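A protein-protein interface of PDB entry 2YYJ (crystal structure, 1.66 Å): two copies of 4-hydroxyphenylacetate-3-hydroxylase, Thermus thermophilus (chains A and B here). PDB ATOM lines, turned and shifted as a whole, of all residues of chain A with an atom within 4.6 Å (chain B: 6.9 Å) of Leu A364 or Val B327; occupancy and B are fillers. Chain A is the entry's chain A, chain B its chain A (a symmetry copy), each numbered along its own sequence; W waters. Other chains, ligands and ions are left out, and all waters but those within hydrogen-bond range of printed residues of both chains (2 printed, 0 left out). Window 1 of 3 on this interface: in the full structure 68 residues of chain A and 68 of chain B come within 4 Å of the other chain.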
ATOM      1  N   PHE A 335       4.205  22.050   8.224  1.00  0.00           N
ATOM      2  CA  PHE A 335       5.582  22.037   8.711  1.00  0.00           C
ATOM      3  C   PHE A 335       5.656  21.212   9.993  1.00  0.00           C
ATOM      4  O   PHE A 335       6.585  20.435  10.194  1.00  0.00           O
ATOM      5  CB  PHE A 335       6.070  23.456   9.021  1.00  0.00           C
ATOM      6  CG  PHE A 335       6.478  24.251   7.812  1.00  0.00           C
ATOM      7  CD1 PHE A 335       7.395  23.741   6.898  1.00  0.00           C
ATOM      8  CD2 PHE A 335       6.000  25.548   7.630  1.00  0.00           C
ATOM      9  CE1 PHE A 335       7.838  24.516   5.819  1.00  0.00           C
ATOM     10  CE2 PHE A 335       6.434  26.329   6.559  1.00  0.00           C
ATOM     11  CZ  PHE A 335       7.355  25.813   5.653  1.00  0.00           C
ATOM     12  N   GLY A 360      11.978  25.749   7.681  1.00  0.00           N
ATOM     13  CA  GLY A 360      10.982  26.328   6.799  1.00  0.00           C
ATOM     14  C   GLY A 360       9.986  27.142   7.605  1.00  0.00           C
ATOM     15  O   GLY A 360       9.705  28.294   7.281  1.00  0.00           O
ATOM     16  N   ALA A 361       9.463  26.548   8.672  1.00  0.00           N
ATOM     17  CA  ALA A 361       8.488  27.230   9.518  1.00  0.00           C
ATOM     18  C   ALA A 361       9.024  28.492  10.192  1.00  0.00           C
ATOM     19  O   ALA A 361       8.374  29.537  10.157  1.00  0.00           O
ATOM     20  CB  ALA A 361       7.960  26.270  10.583  1.00  0.00           C
ATOM     21  N   ARG A 362      10.203  28.404  10.804  1.00  0.00           N
ATOM     22  CA  ARG A 362      10.750  29.562  11.513  1.00  0.00           C
ATOM     23  C   ARG A 362      11.273  30.675  10.612  1.00  0.00           C
ATOM     24  O   ARG A 362      11.470  31.802  11.064  1.00  0.00           O
ATOM     25  CB  ARG A 362      11.823  29.115  12.519  1.00  0.00           C
ATOM     26  CG  ARG A 362      13.143  28.644  11.929  1.00  0.00           C
ATOM     27  CD  ARG A 362      13.880  27.747  12.927  1.00  0.00           C
ATOM     28  NE  ARG A 362      15.232  27.431  12.478  1.00  0.00           N
ATOM     29  CZ  ARG A 362      16.323  28.070  12.885  1.00  0.00           C
ATOM     30  NH1 ARG A 362      16.225  29.063  13.764  1.00  0.00           N
ATOM     31  NH2 ARG A 362      17.510  27.729  12.399  1.00  0.00           N
ATOM     32  N   ASN A 363      11.486  30.369   9.336  1.00  0.00           N
ATOM     33  CA  ASN A 363      11.941  31.387   8.400  1.00  0.00           C
ATOM     34  C   ASN A 363      10.778  31.912   7.564  1.00  0.00           C
ATOM     35  O   ASN A 363      10.883  32.962   6.927  1.00  0.00           O
ATOM     36  CB  ASN A 363      13.052  30.834   7.503  1.00  0.00           C
ATOM     37  CG  ASN A 363      14.388  30.782   8.216  1.00  0.00           C
ATOM     38  OD1 ASN A 363      14.940  29.707   8.471  1.00  0.00           O
ATOM     39  ND2 ASN A 363      14.910  31.952   8.556  1.00  0.00           N
ATOM     40  N   LEU A 364       9.657  31.193   7.571  1.00  0.00           N
ATOM     41  CA  LEU A 364       8.500  31.654   6.815  1.00  0.00           C
ATOM     42  C   LEU A 364       7.534  32.455   7.683  1.00  0.00           C
ATOM     43  O   LEU A 364       7.019  33.481   7.247  1.00  0.00           O
ATOM     44  CB  LEU A 364       7.744  30.481   6.172  1.00  0.00           C
ATOM     45  CG  LEU A 364       6.567  30.909   5.277  1.00  0.00           C
ATOM     46  CD1 LEU A 364       7.075  31.752   4.107  1.00  0.00           C
ATOM     47  CD2 LEU A 364       5.835  29.679   4.759  1.00  0.00           C
ATOM     48  N   TYR A 365       7.295  32.011   8.915  1.00  0.00           N
ATOM     49  CA  TYR A 365       6.344  32.722   9.768  1.00  0.00           C
ATOM     50  C   TYR A 365       6.663  34.199  10.016  1.00  0.00           C
ATOM     51  O   TYR A 365       5.751  35.021  10.103  1.00  0.00           O
ATOM     52  CB  TYR A 365       6.153  32.000  11.105  1.00  0.00           C
ATOM     53  CG  TYR A 365       4.814  32.328  11.725  1.00  0.00           C
ATOM     54  CD1 TYR A 365       3.628  31.878  11.141  1.00  0.00           C
ATOM     55  CD2 TYR A 365       4.726  33.131  12.860  1.00  0.00           C
ATOM     56  CE1 TYR A 365       2.382  32.222  11.677  1.00  0.00           C
ATOM     57  CE2 TYR A 365       3.493  33.482  13.401  1.00  0.00           C
ATOM     58  CZ  TYR A 365       2.327  33.026  12.807  1.00  0.00           C
ATOM     59  OH  TYR A 365       1.109  33.370  13.349  1.00  0.00           O
ATOM     60  N   PRO A 366       7.952  34.560  10.153  1.00  0.00           N
ATOM     61  CA  PRO A 366       8.253  35.980  10.380  1.00  0.00           C
ATOM     62  C   PRO A 366       7.761  36.845   9.215  1.00  0.00           C
ATOM     63  O   PRO A 366       7.587  38.059   9.359  1.00  0.00           O
ATOM     64  CB  PRO A 366       9.774  35.993  10.514  1.00  0.00           C
ATOM     65  CG  PRO A 366      10.050  34.667  11.161  1.00  0.00           C
ATOM     66  CD  PRO A 366       9.150  33.730  10.370  1.00  0.00           C
ATOM     67  N   ARG A 367       7.553  36.215   8.059  1.00  0.00           N
ATOM     68  CA  ARG A 367       7.059  36.912   6.873  1.00  0.00           C
ATOM     69  C   ARG A 367       5.533  36.888   6.844  1.00  0.00           C
ATOM     70  O   ARG A 367       4.892  37.854   6.421  1.00  0.00           O
ATOM     71  CB  ARG A 367       7.586  36.248   5.597  1.00  0.00           C
ATOM     72  CG  ARG A 367       9.099  36.272   5.444  1.00  0.00           C
ATOM     73  CD  ARG A 367       9.537  35.391   4.280  1.00  0.00           C
ATOM     74  NE  ARG A 367       9.168  35.953   2.983  1.00  0.00           N
ATOM     75  CZ  ARG A 367       9.861  36.895   2.351  1.00  0.00           C
ATOM     76  NH1 ARG A 367      10.967  37.385   2.895  1.00  0.00           N
ATOM     77  NH2 ARG A 367       9.446  37.352   1.177  1.00  0.00           N
ATOM     78  N   LEU A 368       4.953  35.780   7.295  1.00  0.00           N
ATOM     79  CA  LEU A 368       3.504  35.626   7.304  1.00  0.00           C
ATOM     80  C   LEU A 368       2.799  36.432   8.385  1.00  0.00           C
ATOM     81  O   LEU A 368       1.736  37.006   8.143  1.00  0.00           O
ATOM     82  CB  LEU A 368       3.125  34.151   7.476  1.00  0.00           C
ATOM     83  CG  LEU A 368       3.725  33.137   6.497  1.00  0.00           C
ATOM     84  CD1 LEU A 368       3.127  31.765   6.791  1.00  0.00           C
ATOM     85  CD2 LEU A 368       3.436  33.544   5.061  1.00  0.00           C
ATOM     86  N   TYR A 449      18.500  33.706   7.090  1.00  0.00           N
ATOM     87  CA  TYR A 449      18.457  33.226   5.714  1.00  0.00           C
ATOM     88  C   TYR A 449      19.854  32.885   5.208  1.00  0.00           C
ATOM     89  O   TYR A 449      20.042  31.890   4.506  1.00  0.00           O
ATOM     90  CB  TYR A 449      17.776  34.258   4.809  1.00  0.00           C
ATOM     91  CG  TYR A 449      16.274  34.073   4.745  1.00  0.00           C
ATOM     92  CD1 TYR A 449      15.496  34.087   5.904  1.00  0.00           C
ATOM     93  CD2 TYR A 449      15.636  33.841   3.526  1.00  0.00           C
ATOM     94  CE1 TYR A 449      14.119  33.870   5.851  1.00  0.00           C
ATOM     95  CE2 TYR A 449      14.259  33.620   3.461  1.00  0.00           C
ATOM     96  CZ  TYR A 449      13.508  33.634   4.622  1.00  0.00           C
ATOM     97  OH  TYR A 449      12.148  33.403   4.551  1.00  0.00           O
ATOM     98  N   LEU A 452      20.703  29.567   6.668  1.00  0.00           N
ATOM     99  CA  LEU A 452      20.035  28.472   5.969  1.00  0.00           C
ATOM    100  C   LEU A 452      20.748  28.165   4.653  1.00  0.00           C
ATOM    101  O   LEU A 452      20.986  27.005   4.316  1.00  0.00           O
ATOM    102  CB  LEU A 452      18.566  28.830   5.707  1.00  0.00           C
ATOM    103  CG  LEU A 452      17.738  27.815   4.912  1.00  0.00           C
ATOM    104  CD1 LEU A 452      17.767  26.459   5.608  1.00  0.00           C
ATOM    105  CD2 LEU A 452      16.303  28.319   4.769  1.00  0.00           C
ATOM    106  N   THR B 296      10.185  23.311  -8.004  1.00  0.00           N
ATOM    107  CA  THR B 296      10.938  24.168  -7.094  1.00  0.00           C
ATOM    108  C   THR B 296      12.373  23.653  -6.932  1.00  0.00           C
ATOM    109  O   THR B 296      13.316  24.441  -6.832  1.00  0.00           O
ATOM    110  CB  THR B 296      10.239  24.257  -5.723  1.00  0.00           C
ATOM    111  OG1 THR B 296       8.866  24.633  -5.920  1.00  0.00           O
ATOM    112  CG2 THR B 296      10.912  25.308  -4.846  1.00  0.00           C
ATOM    113  N   ILE B 322      18.414  32.646  -2.449  1.00  0.00           N
ATOM    114  CA  ILE B 322      18.450  31.205  -2.657  1.00  0.00           C
ATOM    115  C   ILE B 322      17.802  30.515  -1.456  1.00  0.00           C
ATOM    116  O   ILE B 322      17.062  29.542  -1.614  1.00  0.00           O
ATOM    117  CB  ILE B 322      19.903  30.720  -2.880  1.00  0.00           C
ATOM    118  CG1 ILE B 322      20.409  31.275  -4.219  1.00  0.00           C
ATOM    119  CG2 ILE B 322      19.966  29.191  -2.861  1.00  0.00           C
ATOM    120  CD1 ILE B 322      21.886  31.051  -4.487  1.00  0.00           C
ATOM    121  N   ALA B 323      18.052  31.039  -0.259  1.00  0.00           N
ATOM    122  CA  ALA B 323      17.458  30.469   0.949  1.00  0.00           C
ATOM    123  C   ALA B 323      15.934  30.608   0.899  1.00  0.00           C
ATOM    124  O   ALA B 323      15.205  29.768   1.429  1.00  0.00           O
ATOM    125  CB  ALA B 323      18.012  31.171   2.189  1.00  0.00           C
ATOM    126  N   GLU B 324      15.454  31.671   0.260  1.00  0.00           N
ATOM    127  CA  GLU B 324      14.018  31.887   0.141  1.00  0.00           C
ATOM    128  C   GLU B 324      13.414  30.743  -0.680  1.00  0.00           C
ATOM    129  O   GLU B 324      12.346  30.222  -0.350  1.00  0.00           O
ATOM    130  CB  GLU B 324      13.745  33.236  -0.534  1.00  0.00           C
ATOM    131  CG  GLU B 324      12.367  33.792  -0.256  1.00  0.00           C
ATOM    132  CD  GLU B 324      12.159  35.166  -0.865  1.00  0.00           C
ATOM    133  OE1 GLU B 324      13.092  35.996  -0.805  1.00  0.00           O
ATOM    134  OE2 GLU B 324      11.056  35.416  -1.391  1.00  0.00           O
ATOM    135  N   ILE B 325      14.102  30.342  -1.746  1.00  0.00           N
ATOM    136  CA  ILE B 325      13.613  29.242  -2.571  1.00  0.00           C
ATOM    137  C   ILE B 325      13.606  27.965  -1.725  1.00  0.00           C
ATOM    138  O   ILE B 325      12.705  27.140  -1.837  1.00  0.00           O
ATOM    139  CB  ILE B 325      14.505  29.025  -3.826  1.00  0.00           C
ATOM    140  CG1 ILE B 325      14.429  30.257  -4.735  1.00  0.00           C
ATOM    141  CG2 ILE B 325      14.052  27.775  -4.587  1.00  0.00           C
ATOM    142  CD1 ILE B 325      15.263  30.142  -6.006  1.00  0.00           C
ATOM    143  N   ILE B 326      14.615  27.810  -0.870  1.00  0.00           N
ATOM    144  CA  ILE B 326      14.697  26.639  -0.002  1.00  0.00           C
ATOM    145  C   ILE B 326      13.503  26.608   0.951  1.00  0.00           C
ATOM    146  O   ILE B 326      12.924  25.551   1.199  1.00  0.00           O
ATOM    147  CB  ILE B 326      16.014  26.641   0.813  1.00  0.00           C
ATOM    148  CG1 ILE B 326      17.200  26.429  -0.133  1.00  0.00           C
ATOM    149  CG2 ILE B 326      15.986  25.538   1.870  1.00  0.00           C
ATOM    150  CD1 ILE B 326      18.557  26.674   0.512  1.00  0.00           C
ATOM    151  N   VAL B 327      13.133  27.771   1.482  1.00  0.00           N
ATOM    152  CA  VAL B 327      11.994  27.849   2.390  1.00  0.00           C
ATOM    153  C   VAL B 327      10.731  27.399   1.656  1.00  0.00           C
ATOM    154  O   VAL B 327       9.936  26.621   2.188  1.00  0.00           O
ATOM    155  CB  VAL B 327      11.795  29.293   2.921  1.00  0.00           C
ATOM    156  CG1 VAL B 327      10.474  29.401   3.686  1.00  0.00           C
ATOM    157  CG2 VAL B 327      12.958  29.671   3.833  1.00  0.00           C
ATOM    158  N   TYR B 328      10.555  27.876   0.427  1.00  0.00           N
ATOM    159  CA  TYR B 328       9.380  27.506  -0.354  1.00  0.00           C
ATOM    160  C   TYR B 328       9.388  26.019  -0.697  1.00  0.00           C
ATOM    161  O   TYR B 328       8.338  25.372  -0.707  1.00  0.00           O
ATOM    162  CB  TYR B 328       9.298  28.351  -1.631  1.00  0.00           C
ATOM    163  CG  TYR B 328       9.242  29.841  -1.365  1.00  0.00           C
ATOM    164  CD1 TYR B 328       8.755  30.337  -0.155  1.00  0.00           C
ATOM    165  CD2 TYR B 328       9.671  30.759  -2.327  1.00  0.00           C
ATOM    166  CE1 TYR B 328       8.698  31.707   0.094  1.00  0.00           C
ATOM    167  CE2 TYR B 328       9.615  32.136  -2.086  1.00  0.00           C
ATOM    168  CZ  TYR B 328       9.129  32.599  -0.874  1.00  0.00           C
ATOM    169  OH  TYR B 328       9.072  33.954  -0.625  1.00  0.00           O
ATOM    170  N   LEU B 329      10.569  25.477  -0.981  1.00  0.00           N
ATOM    171  CA  LEU B 329      10.686  24.053  -1.286  1.00  0.00           C
ATOM    172  C   LEU B 329      10.239  23.239  -0.074  1.00  0.00           C
ATOM    173  O   LEU B 329       9.474  22.281  -0.205  1.00  0.00           O
ATOM    174  CB  LEU B 329      12.133  23.697  -1.636  1.00  0.00           C
ATOM    175  CG  LEU B 329      12.466  22.204  -1.754  1.00  0.00           C
ATOM    176  CD1 LEU B 329      11.584  21.542  -2.816  1.00  0.00           C
ATOM    177  CD2 LEU B 329      13.939  22.047  -2.108  1.00  0.00           C
ATOM    178  N   GLU B 330      10.716  23.621   1.108  1.00  0.00           N
ATOM    179  CA  GLU B 330      10.345  22.907   2.322  1.00  0.00           C
ATOM    180  C   GLU B 330       8.847  23.033   2.599  1.00  0.00           C
ATOM    181  O   GLU B 330       8.224  22.094   3.095  1.00  0.00           O
ATOM    182  CB  GLU B 330      11.161  23.424   3.512  1.00  0.00           C
ATOM    183  CG  GLU B 330      12.641  23.028   3.476  1.00  0.00           C
ATOM    184  CD  GLU B 330      12.864  21.520   3.563  1.00  0.00           C
ATOM    185  OE1 GLU B 330      12.060  20.831   4.224  1.00  0.00           O
ATOM    186  OE2 GLU B 330      13.856  21.021   2.985  1.00  0.00           O
ATOM    187  N   ALA B 331       8.263  24.183   2.270  1.00  0.00           N
ATOM    188  CA  ALA B 331       6.832  24.381   2.474  1.00  0.00           C
ATOM    189  C   ALA B 331       6.048  23.381   1.621  1.00  0.00           C
ATOM    190  O   ALA B 331       5.100  22.751   2.096  1.00  0.00           O
ATOM    191  CB  ALA B 331       6.433  25.811   2.099  1.00  0.00           C
ATOM    192  N   MET B 332       6.443  23.230   0.362  1.00  0.00           N
ATOM    193  CA  MET B 332       5.744  22.304  -0.521  1.00  0.00           C
ATOM    194  C   MET B 332       5.945  20.858  -0.068  1.00  0.00           C
ATOM    195  O   MET B 332       5.014  20.051  -0.121  1.00  0.00           O
ATOM    196  CB  MET B 332       6.202  22.502  -1.971  1.00  0.00           C
ATOM    197  CG  MET B 332       5.893  23.895  -2.523  1.00  0.00           C
ATOM    198  SD  MET B 332       4.157  24.390  -2.302  1.00  0.00           S
ATOM    199  CE  MET B 332       3.400  23.511  -3.629  1.00  0.00           C
ATOM    200  N   LEU B 364      -1.169  28.421  -2.235  1.00  0.00           N
ATOM    201  CA  LEU B 364       0.040  29.148  -1.872  1.00  0.00           C
ATOM    202  C   LEU B 364       1.043  29.195  -3.021  1.00  0.00           C
ATOM    203  O   LEU B 364       1.649  30.235  -3.269  1.00  0.00           O
ATOM    204  CB  LEU B 364       0.718  28.534  -0.637  1.00  0.00           C
ATOM    205  CG  LEU B 364       1.947  29.317  -0.143  1.00  0.00           C
ATOM    206  CD1 LEU B 364       1.539  30.727   0.280  1.00  0.00           C
ATOM    207  CD2 LEU B 364       2.594  28.585   1.024  1.00  0.00           C
ATOM    208  N   LEU B 368       3.887  31.882  -4.623  1.00  0.00           N
ATOM    209  CA  LEU B 368       5.318  31.639  -4.500  1.00  0.00           C
ATOM    210  C   LEU B 368       6.056  31.584  -5.830  1.00  0.00           C
ATOM    211  O   LEU B 368       7.167  32.103  -5.950  1.00  0.00           O
ATOM    212  CB  LEU B 368       5.576  30.328  -3.750  1.00  0.00           C
ATOM    213  CG  LEU B 368       4.924  30.148  -2.376  1.00  0.00           C
ATOM    214  CD1 LEU B 368       5.404  28.828  -1.779  1.00  0.00           C
ATOM    215  CD2 LEU B 368       5.281  31.306  -1.458  1.00  0.00           C
HETATM  216  O   HOH W   1      11.972  38.676   0.092  1.00  0.00           O
HETATM  217  O   HOH W   2       6.471  34.866   1.509  1.00  0.00           O
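OE2 of Glu B324 lies within salt-bridge range of NH2 of Arg A367.
O of Asn A363 lies within hydrogen-bond range of OH of Tyr A449. OE2 of Glu B324 is in hydrogen-bond range of OH of Tyr B328.
CE1 of Phe A335 touches O of Glu B330, at 3.7 Å. Phe A335 touches Ala B331. Gly A360 touches Val B327. CB of Asn A363 touches CG2 of Val B327, 3.9 Å away. Val B327 touches Leu A364. Arg A367 touches Tyr B328 (NH2 to OH, 3.9 Å). Ala B323 touches Tyr A449. Val B327 touches Tyr A449. Leu A452 touches Ala B323. Val B327 touches Leu A452 (CG2 to CD2, 3.7 Å).
Of the printed residues of chain B, Phe A335 touches Glu B330 (3.7 Å) and Ala B331 (3.5 Å). Printed residues of chain B within 4 Å of Gly A360: Val B327 (3.8 Å). Of chain B, only Val B327 (3.8 Å) comes within 4 Å of Leu A364. Of the printed residues of chain A, Ala B323 touches Tyr A449 and Leu A452. Val B327 touches just these residues of chain A: Gly A360 (3.8 Å), Asn A363 (3.9 Å), Leu A364 (3.8 Å), Tyr A449 (3.9 Å) and Leu A452 (3.7 Å). Of the printed residues of chain A, Glu B330 touches Phe A335 (3.7 Å). Printed residues of chain A within 4 Å of Ala B331: Phe A335. Leu B368 touches none of the printed residues of chain A. The nearest residue of chain B that does not touch Leu A364 is Tyr B328 (4.3 Å). The nearest residue of chain A that does not touch Val B327 is Phe A335 (4.4 Å).
Of the 12 printed residues of chain A, 7 touch a printed residue of chain B. Hydrophobic or aromatic side chains of chain A that line the printed part of chain B: Phe A335, Leu A364, Tyr A449 and Leu A452. Of the 14 printed residues of chain B, 6 touch a printed residue of chain A. Printed residues of chain B that touch a printed residue of chain A: Ala B323, Glu B324, Val B327, Tyr B328, Glu B330 and Ala B331. Along chain B the printed residues that touch a printed residue of chain A span positions 323 to 331. Among the printed residues, 12 pairs touch across the chains.
Positions printed for both chains: 364 and 368. Of the 12 pairs that touch across the chains among the printed residues, none has its exchanged pair printed and touching as well.
Water W1 lies within hydrogen-bond range of the side-chain carboxylate (OE1) of Glu B324 (3.0 Å) and the guanidinium group (NH2) of Arg A367 (3.1 Å). Water W2 lies within hydrogen-bond range of NE of Arg A367 (3.3 Å) and OH of Tyr B328 (3.5 Å).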
